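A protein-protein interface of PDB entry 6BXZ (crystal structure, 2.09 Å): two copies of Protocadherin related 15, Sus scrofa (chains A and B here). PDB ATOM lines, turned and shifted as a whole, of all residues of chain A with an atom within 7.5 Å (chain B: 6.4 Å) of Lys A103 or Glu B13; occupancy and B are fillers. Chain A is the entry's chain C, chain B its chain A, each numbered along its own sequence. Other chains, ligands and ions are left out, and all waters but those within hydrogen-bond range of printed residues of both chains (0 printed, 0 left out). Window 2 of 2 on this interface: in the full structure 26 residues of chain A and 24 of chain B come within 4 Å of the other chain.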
ATOM      1  N   PHE A   9      -1.278  24.304 -23.862  1.00  0.00           N
ATOM      2  CA  PHE A   9      -1.114  25.752 -23.932  1.00  0.00           C
ATOM      3  C   PHE A   9      -1.210  26.261 -25.374  1.00  0.00           C
ATOM      4  O   PHE A   9      -0.941  25.531 -26.331  1.00  0.00           O
ATOM      5  CB  PHE A   9       0.221  26.171 -23.319  1.00  0.00           C
ATOM      6  CG  PHE A   9       0.292  26.002 -21.826  1.00  0.00           C
ATOM      7  CD1 PHE A   9      -0.190  26.985 -20.976  1.00  0.00           C
ATOM      8  CD2 PHE A   9       0.882  24.872 -21.269  1.00  0.00           C
ATOM      9  CE1 PHE A   9      -0.109  26.838 -19.599  1.00  0.00           C
ATOM     10  CE2 PHE A   9       0.968  24.719 -19.895  1.00  0.00           C
ATOM     11  CZ  PHE A   9       0.472  25.705 -19.059  1.00  0.00           C
ATOM     12  N   GLN A  11       0.791  28.452 -26.499  1.00  0.00           N
ATOM     13  CA  GLN A  11       2.201  28.557 -26.872  1.00  0.00           C
ATOM     14  C   GLN A  11       3.049  27.648 -25.979  1.00  0.00           C
ATOM     15  O   GLN A  11       2.710  27.424 -24.815  1.00  0.00           O
ATOM     16  CB  GLN A  11       2.686  30.001 -26.722  1.00  0.00           C
ATOM     17  CG  GLN A  11       1.805  31.064 -27.370  1.00  0.00           C
ATOM     18  CD  GLN A  11       2.331  32.479 -27.138  1.00  0.00           C
ATOM     19  OE1 GLN A  11       3.426  32.674 -26.615  1.00  0.00           O
ATOM     20  NE2 GLN A  11       1.539  33.476 -27.524  1.00  0.00           N
ATOM     21  N   GLU A  12       4.157  27.146 -26.518  1.00  0.00           N
ATOM     22  CA  GLU A  12       5.082  26.303 -25.746  1.00  0.00           C
ATOM     23  C   GLU A  12       5.745  27.082 -24.597  1.00  0.00           C
ATOM     24  O   GLU A  12       5.907  26.555 -23.494  1.00  0.00           O
ATOM     25  CB  GLU A  12       6.146  25.697 -26.662  1.00  0.00           C
ATOM     26  CG  GLU A  12       5.548  24.720 -27.673  1.00  0.00           C
ATOM     27  CD  GLU A  12       6.469  24.327 -28.819  1.00  0.00           C
ATOM     28  OE1 GLU A  12       6.061  23.417 -29.590  1.00  0.00           O
ATOM     29  OE2 GLU A  12       7.582  24.895 -28.980  1.00  0.00           O
ATOM     30  N   GLU A  13       6.119  28.328 -24.873  1.00  0.00           N
ATOM     31  CA  GLU A  13       6.604  29.269 -23.861  1.00  0.00           C
ATOM     32  C   GLU A  13       6.024  30.657 -24.137  1.00  0.00           C
ATOM     33  O   GLU A  13       5.576  30.927 -25.246  1.00  0.00           O
ATOM     34  CB  GLU A  13       8.141  29.307 -23.852  1.00  0.00           C
ATOM     35  CG  GLU A  13       8.785  29.530 -25.205  1.00  0.00           C
ATOM     36  CD  GLU A  13      10.306  29.359 -25.166  1.00  0.00           C
ATOM     37  OE1 GLU A  13      10.839  28.471 -24.454  1.00  0.00           O
ATOM     38  OE2 GLU A  13      10.988  30.111 -25.868  1.00  0.00           O
ATOM     39  N   TYR A  14       6.020  31.522 -23.130  1.00  0.00           N
ATOM     40  CA  TYR A  14       5.458  32.864 -23.252  1.00  0.00           C
ATOM     41  C   TYR A  14       6.563  33.911 -23.051  1.00  0.00           C
ATOM     42  O   TYR A  14       7.393  33.789 -22.150  1.00  0.00           O
ATOM     43  CB  TYR A  14       4.323  33.065 -22.251  1.00  0.00           C
ATOM     44  CG  TYR A  14       3.100  32.230 -22.563  1.00  0.00           C
ATOM     45  CD1 TYR A  14       3.074  30.870 -22.262  1.00  0.00           C
ATOM     46  CD2 TYR A  14       1.975  32.795 -23.167  1.00  0.00           C
ATOM     47  CE1 TYR A  14       1.964  30.088 -22.552  1.00  0.00           C
ATOM     48  CE2 TYR A  14       0.854  32.025 -23.460  1.00  0.00           C
ATOM     49  CZ  TYR A  14       0.849  30.665 -23.146  1.00  0.00           C
ATOM     50  OH  TYR A  14      -0.255  29.874 -23.420  1.00  0.00           O
ATOM     51  N   ARG A  15       6.559  34.915 -23.917  1.00  0.00           N
ATOM     52  CA  ARG A  15       7.460  36.055 -23.834  1.00  0.00           C
ATOM     53  C   ARG A  15       6.625  37.308 -24.000  1.00  0.00           C
ATOM     54  O   ARG A  15       6.565  37.861 -25.092  1.00  0.00           O
ATOM     55  CB  ARG A  15       8.559  35.986 -24.907  1.00  0.00           C
ATOM     56  CG  ARG A  15       9.578  34.893 -24.660  1.00  0.00           C
ATOM     57  CD  ARG A  15      11.007  35.325 -25.028  1.00  0.00           C
ATOM     58  NE  ARG A  15      11.997  34.334 -24.612  1.00  0.00           N
ATOM     59  CZ  ARG A  15      12.143  33.130 -25.171  1.00  0.00           C
ATOM     60  NH1 ARG A  15      11.375  32.741 -26.195  1.00  0.00           N
ATOM     61  NH2 ARG A  15      13.067  32.273 -24.733  1.00  0.00           N
ATOM     62  N   PRO A  16       5.951  37.743 -22.923  1.00  0.00           N
ATOM     63  CA  PRO A  16       5.115  38.933 -23.033  1.00  0.00           C
ATOM     64  C   PRO A  16       5.977  40.198 -23.149  1.00  0.00           C
ATOM     65  O   PRO A  16       7.194  40.135 -22.920  1.00  0.00           O
ATOM     66  CB  PRO A  16       4.316  38.914 -21.723  1.00  0.00           C
ATOM     67  CG  PRO A  16       5.223  38.245 -20.757  1.00  0.00           C
ATOM     68  CD  PRO A  16       5.902  37.171 -21.564  1.00  0.00           C
ATOM     69  N   ILE A  32      -1.948  33.833 -20.021  1.00  0.00           N
ATOM     70  CA  ILE A  32      -1.644  32.409 -20.182  1.00  0.00           C
ATOM     71  C   ILE A  32      -2.964  31.688 -20.460  1.00  0.00           C
ATOM     72  O   ILE A  32      -3.959  31.925 -19.772  1.00  0.00           O
ATOM     73  CB  ILE A  32      -1.003  31.825 -18.904  1.00  0.00           C
ATOM     74  CG1 ILE A  32       0.239  32.625 -18.491  1.00  0.00           C
ATOM     75  CG2 ILE A  32      -0.654  30.351 -19.083  1.00  0.00           C
ATOM     76  CD1 ILE A  32       1.277  32.839 -19.584  1.00  0.00           C
ATOM     77  N   VAL A  78      12.091  34.336 -14.807  1.00  0.00           N
ATOM     78  CA  VAL A  78      11.664  33.162 -15.566  1.00  0.00           C
ATOM     79  C   VAL A  78      10.719  32.348 -14.671  1.00  0.00           C
ATOM     80  O   VAL A  78      11.165  31.687 -13.728  1.00  0.00           O
ATOM     81  CB  VAL A  78      12.853  32.358 -16.156  1.00  0.00           C
ATOM     82  CG1 VAL A  78      13.924  32.034 -15.116  1.00  0.00           C
ATOM     83  CG2 VAL A  78      12.350  31.097 -16.856  1.00  0.00           C
ATOM     84  N   LEU A  79       9.419  32.452 -14.959  1.00  0.00           N
ATOM     85  CA  LEU A  79       8.378  31.752 -14.220  1.00  0.00           C
ATOM     86  C   LEU A  79       8.003  30.467 -14.933  1.00  0.00           C
ATOM     87  O   LEU A  79       8.036  30.418 -16.169  1.00  0.00           O
ATOM     88  CB  LEU A  79       7.111  32.610 -14.110  1.00  0.00           C
ATOM     89  CG  LEU A  79       7.210  34.027 -13.542  1.00  0.00           C
ATOM     90  CD1 LEU A  79       5.814  34.621 -13.441  1.00  0.00           C
ATOM     91  CD2 LEU A  79       7.909  34.010 -12.189  1.00  0.00           C
ATOM     92  N   ARG A  80       7.647  29.440 -14.159  1.00  0.00           N
ATOM     93  CA  ARG A  80       6.958  28.270 -14.700  1.00  0.00           C
ATOM     94  C   ARG A  80       5.518  28.381 -14.233  1.00  0.00           C
ATOM     95  O   ARG A  80       5.271  28.442 -13.025  1.00  0.00           O
ATOM     96  CB  ARG A  80       7.553  26.965 -14.177  1.00  0.00           C
ATOM     97  CG  ARG A  80       8.988  26.655 -14.552  1.00  0.00           C
ATOM     98  CD  ARG A  80       9.281  25.178 -14.284  1.00  0.00           C
ATOM     99  NE  ARG A  80       8.634  24.358 -15.308  1.00  0.00           N
ATOM    100  CZ  ARG A  80       9.136  24.071 -16.512  1.00  0.00           C
ATOM    101  NH1 ARG A  80       8.426  23.325 -17.353  1.00  0.00           N
ATOM    102  NH2 ARG A  80      10.335  24.497 -16.890  1.00  0.00           N
ATOM    103  N   VAL A  81       4.583  28.443 -15.181  1.00  0.00           N
ATOM    104  CA  VAL A  81       3.159  28.412 -14.859  1.00  0.00           C
ATOM    105  C   VAL A  81       2.624  27.011 -15.119  1.00  0.00           C
ATOM    106  O   VAL A  81       3.102  26.312 -16.012  1.00  0.00           O
ATOM    107  CB  VAL A  81       2.314  29.461 -15.615  1.00  0.00           C
ATOM    108  CG1 VAL A  81       2.875  30.864 -15.378  1.00  0.00           C
ATOM    109  CG2 VAL A  81       2.221  29.150 -17.106  1.00  0.00           C
ATOM    110  N   THR A 101       2.896  22.283 -17.786  1.00  0.00           N
ATOM    111  CA  THR A 101       3.532  23.563 -17.472  1.00  0.00           C
ATOM    112  C   THR A 101       4.071  24.261 -18.710  1.00  0.00           C
ATOM    113  O   THR A 101       4.136  23.689 -19.795  1.00  0.00           O
ATOM    114  CB  THR A 101       4.661  23.410 -16.420  1.00  0.00           C
ATOM    115  OG1 THR A 101       5.761  22.679 -16.973  1.00  0.00           O
ATOM    116  CG2 THR A 101       4.152  22.690 -15.172  1.00  0.00           C
ATOM    117  N   ALA A 102       4.425  25.526 -18.530  1.00  0.00           N
ATOM    118  CA  ALA A 102       5.024  26.332 -19.590  1.00  0.00           C
ATOM    119  C   ALA A 102       5.829  27.470 -18.975  1.00  0.00           C
ATOM    120  O   ALA A 102       5.486  28.003 -17.915  1.00  0.00           O
ATOM    121  CB  ALA A 102       3.953  26.863 -20.533  1.00  0.00           C
ATOM    122  N   LYS A 103       6.923  27.827 -19.647  1.00  0.00           N
ATOM    123  CA  LYS A 103       7.819  28.867 -19.157  1.00  0.00           C
ATOM    124  C   LYS A 103       7.285  30.229 -19.582  1.00  0.00           C
ATOM    125  O   LYS A 103       6.750  30.370 -20.684  1.00  0.00           O
ATOM    126  CB  LYS A 103       9.241  28.623 -19.665  1.00  0.00           C
ATOM    127  CG  LYS A 103       9.817  27.270 -19.245  1.00  0.00           C
ATOM    128  CD  LYS A 103      11.267  27.108 -19.692  1.00  0.00           C
ATOM    129  CE  LYS A 103      12.206  27.745 -18.682  1.00  0.00           C
ATOM    130  NZ  LYS A 103      13.566  28.003 -19.235  1.00  0.00           N
ATOM    131  N   VAL A 104       7.397  31.214 -18.687  1.00  0.00           N
ATOM    132  CA  VAL A 104       7.062  32.614 -18.986  1.00  0.00           C
ATOM    133  C   VAL A 104       8.313  33.475 -18.745  1.00  0.00           C
ATOM    134  O   VAL A 104       8.754  33.620 -17.602  1.00  0.00           O
ATOM    135  CB  VAL A 104       5.896  33.140 -18.129  1.00  0.00           C
ATOM    136  CG1 VAL A 104       5.485  34.533 -18.584  1.00  0.00           C
ATOM    137  CG2 VAL A 104       4.694  32.207 -18.217  1.00  0.00           C
ATOM    138  N   TYR A 105       8.884  34.020 -19.821  1.00  0.00           N
ATOM    139  CA  TYR A 105      10.054  34.916 -19.712  1.00  0.00           C
ATOM    140  C   TYR A 105       9.557  36.350 -19.556  1.00  0.00           C
ATOM    141  O   TYR A 105       8.997  36.906 -20.495  1.00  0.00           O
ATOM    142  CB  TYR A 105      10.955  34.793 -20.939  1.00  0.00           C
ATOM    143  CG  TYR A 105      11.605  33.432 -21.101  1.00  0.00           C
ATOM    144  CD1 TYR A 105      10.928  32.364 -21.711  1.00  0.00           C
ATOM    145  CD2 TYR A 105      12.894  33.203 -20.622  1.00  0.00           C
ATOM    146  CE1 TYR A 105      11.523  31.108 -21.844  1.00  0.00           C
ATOM    147  CE2 TYR A 105      13.505  31.961 -20.759  1.00  0.00           C
ATOM    148  CZ  TYR A 105      12.825  30.917 -21.364  1.00  0.00           C
ATOM    149  OH  TYR A 105      13.459  29.695 -21.486  1.00  0.00           O
ATOM    150  N   ILE A 106       9.736  36.935 -18.371  1.00  0.00           N
ATOM    151  CA  ILE A 106       9.314  38.313 -18.111  1.00  0.00           C
ATOM    152  C   ILE A 106      10.563  39.215 -18.041  1.00  0.00           C
ATOM    153  O   ILE A 106      11.500  38.923 -17.298  1.00  0.00           O
ATOM    154  CB  ILE A 106       8.509  38.424 -16.800  1.00  0.00           C
ATOM    155  CG1 ILE A 106       7.216  37.595 -16.892  1.00  0.00           C
ATOM    156  CG2 ILE A 106       8.179  39.879 -16.471  1.00  0.00           C
ATOM    157  CD1 ILE A 106       6.514  37.391 -15.567  1.00  0.00           C
ATOM    158  N   GLN B  11      18.303  17.329 -18.468  1.00  0.00           N
ATOM    159  CA  GLN B  11      17.827  18.705 -18.311  1.00  0.00           C
ATOM    160  C   GLN B  11      16.612  18.935 -19.211  1.00  0.00           C
ATOM    161  O   GLN B  11      16.500  18.321 -20.280  1.00  0.00           O
ATOM    162  CB  GLN B  11      18.934  19.692 -18.707  1.00  0.00           C
ATOM    163  CG  GLN B  11      20.301  19.441 -18.075  1.00  0.00           C
ATOM    164  CD  GLN B  11      21.360  20.414 -18.549  1.00  0.00           C
ATOM    165  OE1 GLN B  11      21.067  21.375 -19.248  1.00  0.00           O
ATOM    166  NE2 GLN B  11      22.599  20.168 -18.164  1.00  0.00           N
ATOM    167  N   GLU B  12      15.729  19.845 -18.803  1.00  0.00           N
ATOM    168  CA  GLU B  12      14.559  20.179 -19.625  1.00  0.00           C
ATOM    169  C   GLU B  12      14.947  20.858 -20.946  1.00  0.00           C
ATOM    170  O   GLU B  12      14.364  20.584 -22.001  1.00  0.00           O
ATOM    171  CB  GLU B  12      13.562  21.059 -18.867  1.00  0.00           C
ATOM    172  CG  GLU B  12      12.149  20.854 -19.413  1.00  0.00           C
ATOM    173  CD  GLU B  12      11.134  21.816 -18.843  1.00  0.00           C
ATOM    174  OE1 GLU B  12      11.414  23.040 -18.883  1.00  0.00           O
ATOM    175  OE2 GLU B  12      10.071  21.341 -18.379  1.00  0.00           O
ATOM    176  N   GLU B  13      15.933  21.747 -20.863  1.00  0.00           N
ATOM    177  CA  GLU B  13      16.525  22.398 -22.027  1.00  0.00           C
ATOM    178  C   GLU B  13      18.046  22.474 -21.827  1.00  0.00           C
ATOM    179  O   GLU B  13      18.536  22.380 -20.696  1.00  0.00           O
ATOM    180  CB  GLU B  13      15.925  23.798 -22.232  1.00  0.00           C
ATOM    181  CG  GLU B  13      15.954  24.671 -20.973  1.00  0.00           C
ATOM    182  CD  GLU B  13      15.442  26.065 -21.182  1.00  0.00           C
ATOM    183  OE1 GLU B  13      14.350  26.199 -21.761  1.00  0.00           O
ATOM    184  OE2 GLU B  13      16.134  27.024 -20.744  1.00  0.00           O
ATOM    185  N   TYR B  14      18.779  22.628 -22.928  1.00  0.00           N
ATOM    186  CA  TYR B  14      20.233  22.674 -22.880  1.00  0.00           C
ATOM    187  C   TYR B  14      20.719  24.040 -23.358  1.00  0.00           C
ATOM    188  O   TYR B  14      20.217  24.586 -24.339  1.00  0.00           O
ATOM    189  CB  TYR B  14      20.834  21.554 -23.718  1.00  0.00           C
ATOM    190  CG  TYR B  14      20.593  20.179 -23.132  1.00  0.00           C
ATOM    191  CD1 TYR B  14      19.346  19.556 -23.257  1.00  0.00           C
ATOM    192  CD2 TYR B  14      21.595  19.507 -22.436  1.00  0.00           C
ATOM    193  CE1 TYR B  14      19.111  18.306 -22.718  1.00  0.00           C
ATOM    194  CE2 TYR B  14      21.365  18.244 -21.893  1.00  0.00           C
ATOM    195  CZ  TYR B  14      20.122  17.648 -22.035  1.00  0.00           C
ATOM    196  OH  TYR B  14      19.875  16.387 -21.511  1.00  0.00           O
ATOM    197  N   ARG B  15      21.668  24.596 -22.612  1.00  0.00           N
ATOM    198  CA  ARG B  15      22.289  25.885 -22.931  1.00  0.00           C
ATOM    199  C   ARG B  15      23.794  25.677 -22.787  1.00  0.00           C
ATOM    200  O   ARG B  15      24.370  26.030 -21.760  1.00  0.00           O
ATOM    201  CB  ARG B  15      21.794  26.964 -21.967  1.00  0.00           C
ATOM    202  CG  ARG B  15      20.355  27.375 -22.227  1.00  0.00           C
ATOM    203  CD  ARG B  15      19.761  28.162 -21.072  1.00  0.00           C
ATOM    204  NE  ARG B  15      18.360  28.508 -21.356  1.00  0.00           N
ATOM    205  CZ  ARG B  15      17.961  29.431 -22.230  1.00  0.00           C
ATOM    206  NH1 ARG B  15      18.846  30.119 -22.938  1.00  0.00           N
ATOM    207  NH2 ARG B  15      16.670  29.654 -22.457  1.00  0.00           N
ATOM    208  N   ALA B 102      13.761  17.932 -26.535  1.00  0.00           N
ATOM    209  CA  ALA B 102      14.277  18.992 -25.677  1.00  0.00           C
ATOM    210  C   ALA B 102      14.956  20.083 -26.518  1.00  0.00           C
ATOM    211  O   ALA B 102      15.530  19.800 -27.571  1.00  0.00           O
ATOM    212  CB  ALA B 102      15.249  18.409 -24.662  1.00  0.00           C
ATOM    213  N   LYS B 103      14.874  21.321 -26.059  1.00  0.00           N
ATOM    214  CA  LYS B 103      15.428  22.460 -26.788  1.00  0.00           C
ATOM    215  C   LYS B 103      16.912  22.596 -26.443  1.00  0.00           C
ATOM    216  O   LYS B 103      17.308  22.366 -25.294  1.00  0.00           O
ATOM    217  CB  LYS B 103      14.663  23.749 -26.454  1.00  0.00           C
ATOM    218  CG  LYS B 103      13.162  23.649 -26.707  1.00  0.00           C
ATOM    219  CD  LYS B 103      12.419  24.955 -26.485  1.00  0.00           C
ATOM    220  CE  LYS B 103      12.547  25.882 -27.681  1.00  0.00           C
ATOM    221  NZ  LYS B 103      12.260  27.305 -27.345  1.00  0.00           N
ATOM    222  N   VAL B 104      17.722  22.945 -27.444  1.00  0.00           N
ATOM    223  CA  VAL B 104      19.145  23.272 -27.259  1.00  0.00           C
ATOM    224  C   VAL B 104      19.397  24.695 -27.771  1.00  0.00           C
ATOM    225  O   VAL B 104      19.298  24.950 -28.970  1.00  0.00           O
ATOM    226  CB  VAL B 104      20.081  22.282 -27.992  1.00  0.00           C
ATOM    227  CG1 VAL B 104      21.542  22.569 -27.656  1.00  0.00           C
ATOM    228  CG2 VAL B 104      19.726  20.841 -27.639  1.00  0.00           C
ATOM    229  N   TYR B 105      19.702  25.620 -26.860  1.00  0.00           N
ATOM    230  CA  TYR B 105      20.025  27.011 -27.230  1.00  0.00           C
ATOM    231  C   TYR B 105      21.524  27.118 -27.488  1.00  0.00           C
ATOM    232  O   TYR B 105      22.309  26.992 -26.557  1.00  0.00           O
ATOM    233  CB  TYR B 105      19.607  27.981 -26.123  1.00  0.00           C
ATOM    234  CG  TYR B 105      18.108  28.062 -25.927  1.00  0.00           C
ATOM    235  CD1 TYR B 105      17.437  27.135 -25.104  1.00  0.00           C
ATOM    236  CD2 TYR B 105      17.352  29.062 -26.542  1.00  0.00           C
ATOM    237  CE1 TYR B 105      16.065  27.214 -24.909  1.00  0.00           C
ATOM    238  CE2 TYR B 105      15.972  29.139 -26.351  1.00  0.00           C
ATOM    239  CZ  TYR B 105      15.336  28.218 -25.529  1.00  0.00           C
ATOM    240  OH  TYR B 105      13.972  28.284 -25.338  1.00  0.00           O
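The side-chain carboxylate of Glu A13 is in salt-bridge range of the side-chain amino group of Lys B103, at 3.4 Å. The side-chain hydroxyl (OH) of Tyr B105 lies within hydrogen-bond range of the side-chain carboxylate (OE1) of Glu A13 (3.3 Å). The guanidinium group of Arg A80 lies within salt-bridge range of the side-chain carboxylate of Glu B12, at 2.7 Å. OE2 of Glu B13 lies within salt-bridge range of NZ of Lys A103. The side-chain hydroxyl (OH) of Tyr A105 is in hydrogen-bond range of the guanidinium group (NH2) of Arg B15.
The backbone carbonyl oxygen of Lys A103 is in hydrogen-bond range of the backbone NH of Tyr A14 (2.8 Å). The side-chain hydroxyl of Thr A101 sits at hydrogen-bond distance from the guanidinium group of Arg A80 (2.8 Å). O of Glu B13 sits close to OE1 of Gln B11, 3.1 Å away. The backbone carbonyl oxygen of Lys B103 lies within hydrogen-bond range of the backbone NH of Tyr B14, 2.8 Å away. The backbone carbonyl oxygen (O) of Tyr B14 sits at hydrogen-bond distance from the backbone NH (N) of Tyr B105, at 2.8 Å. The side-chain hydroxyl (OH) of Tyr B105 sits at hydrogen-bond distance from the side-chain amino group (NZ) of Lys B103.
OH of Tyr A105 touches OE1 of Glu B13 (3.6 Å).
Of chain B, only Glu B13 comes within 4 Å of Lys A103. Of the printed residues of chain B, Arg A80 touches Glu B12 (2.7 Å). Printed residues of chain A within 4 Å of Lys B103: Glu A13 (3.4 Å). Printed residues of chain B within 4 Å of Tyr A105: Glu B13 (3.6 Å) and Arg B15 (3.4 Å). The nearest residue of chain A that does not touch Glu B13 is Glu A13 (5.0 Å). The nearest printed residue of chain B that does not touch Arg A80 is Glu B13 (6.5 Å).
Of the 9 printed residues of chain B, 5 touch a printed residue of chain A. Of the 18 printed residues of chain A, 4 touch a printed residue of chain B. Printed residues of chain A that touch a printed residue of chain B: Glu A13, Arg A80, Lys A103 and Tyr A105. Among the printed residues, Asp or Glu carboxylates within 4 Å of a Lys or Arg side-chain nitrogen of the other chain: Glu A13 with Lys B103, Arg A80 with Glu B12 and Lys A103 with Glu B13.
Glu A13 touches Lys B103, and with the chains exchanged Lys A103 touches Glu B13. Glu A13 touches Tyr B105, and with the chains exchanged Tyr A105 touches Glu B13. Tyr A105 touches Arg B15, but with the chains exchanged Arg A15 does not touch Tyr B105 (4.1 Å).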
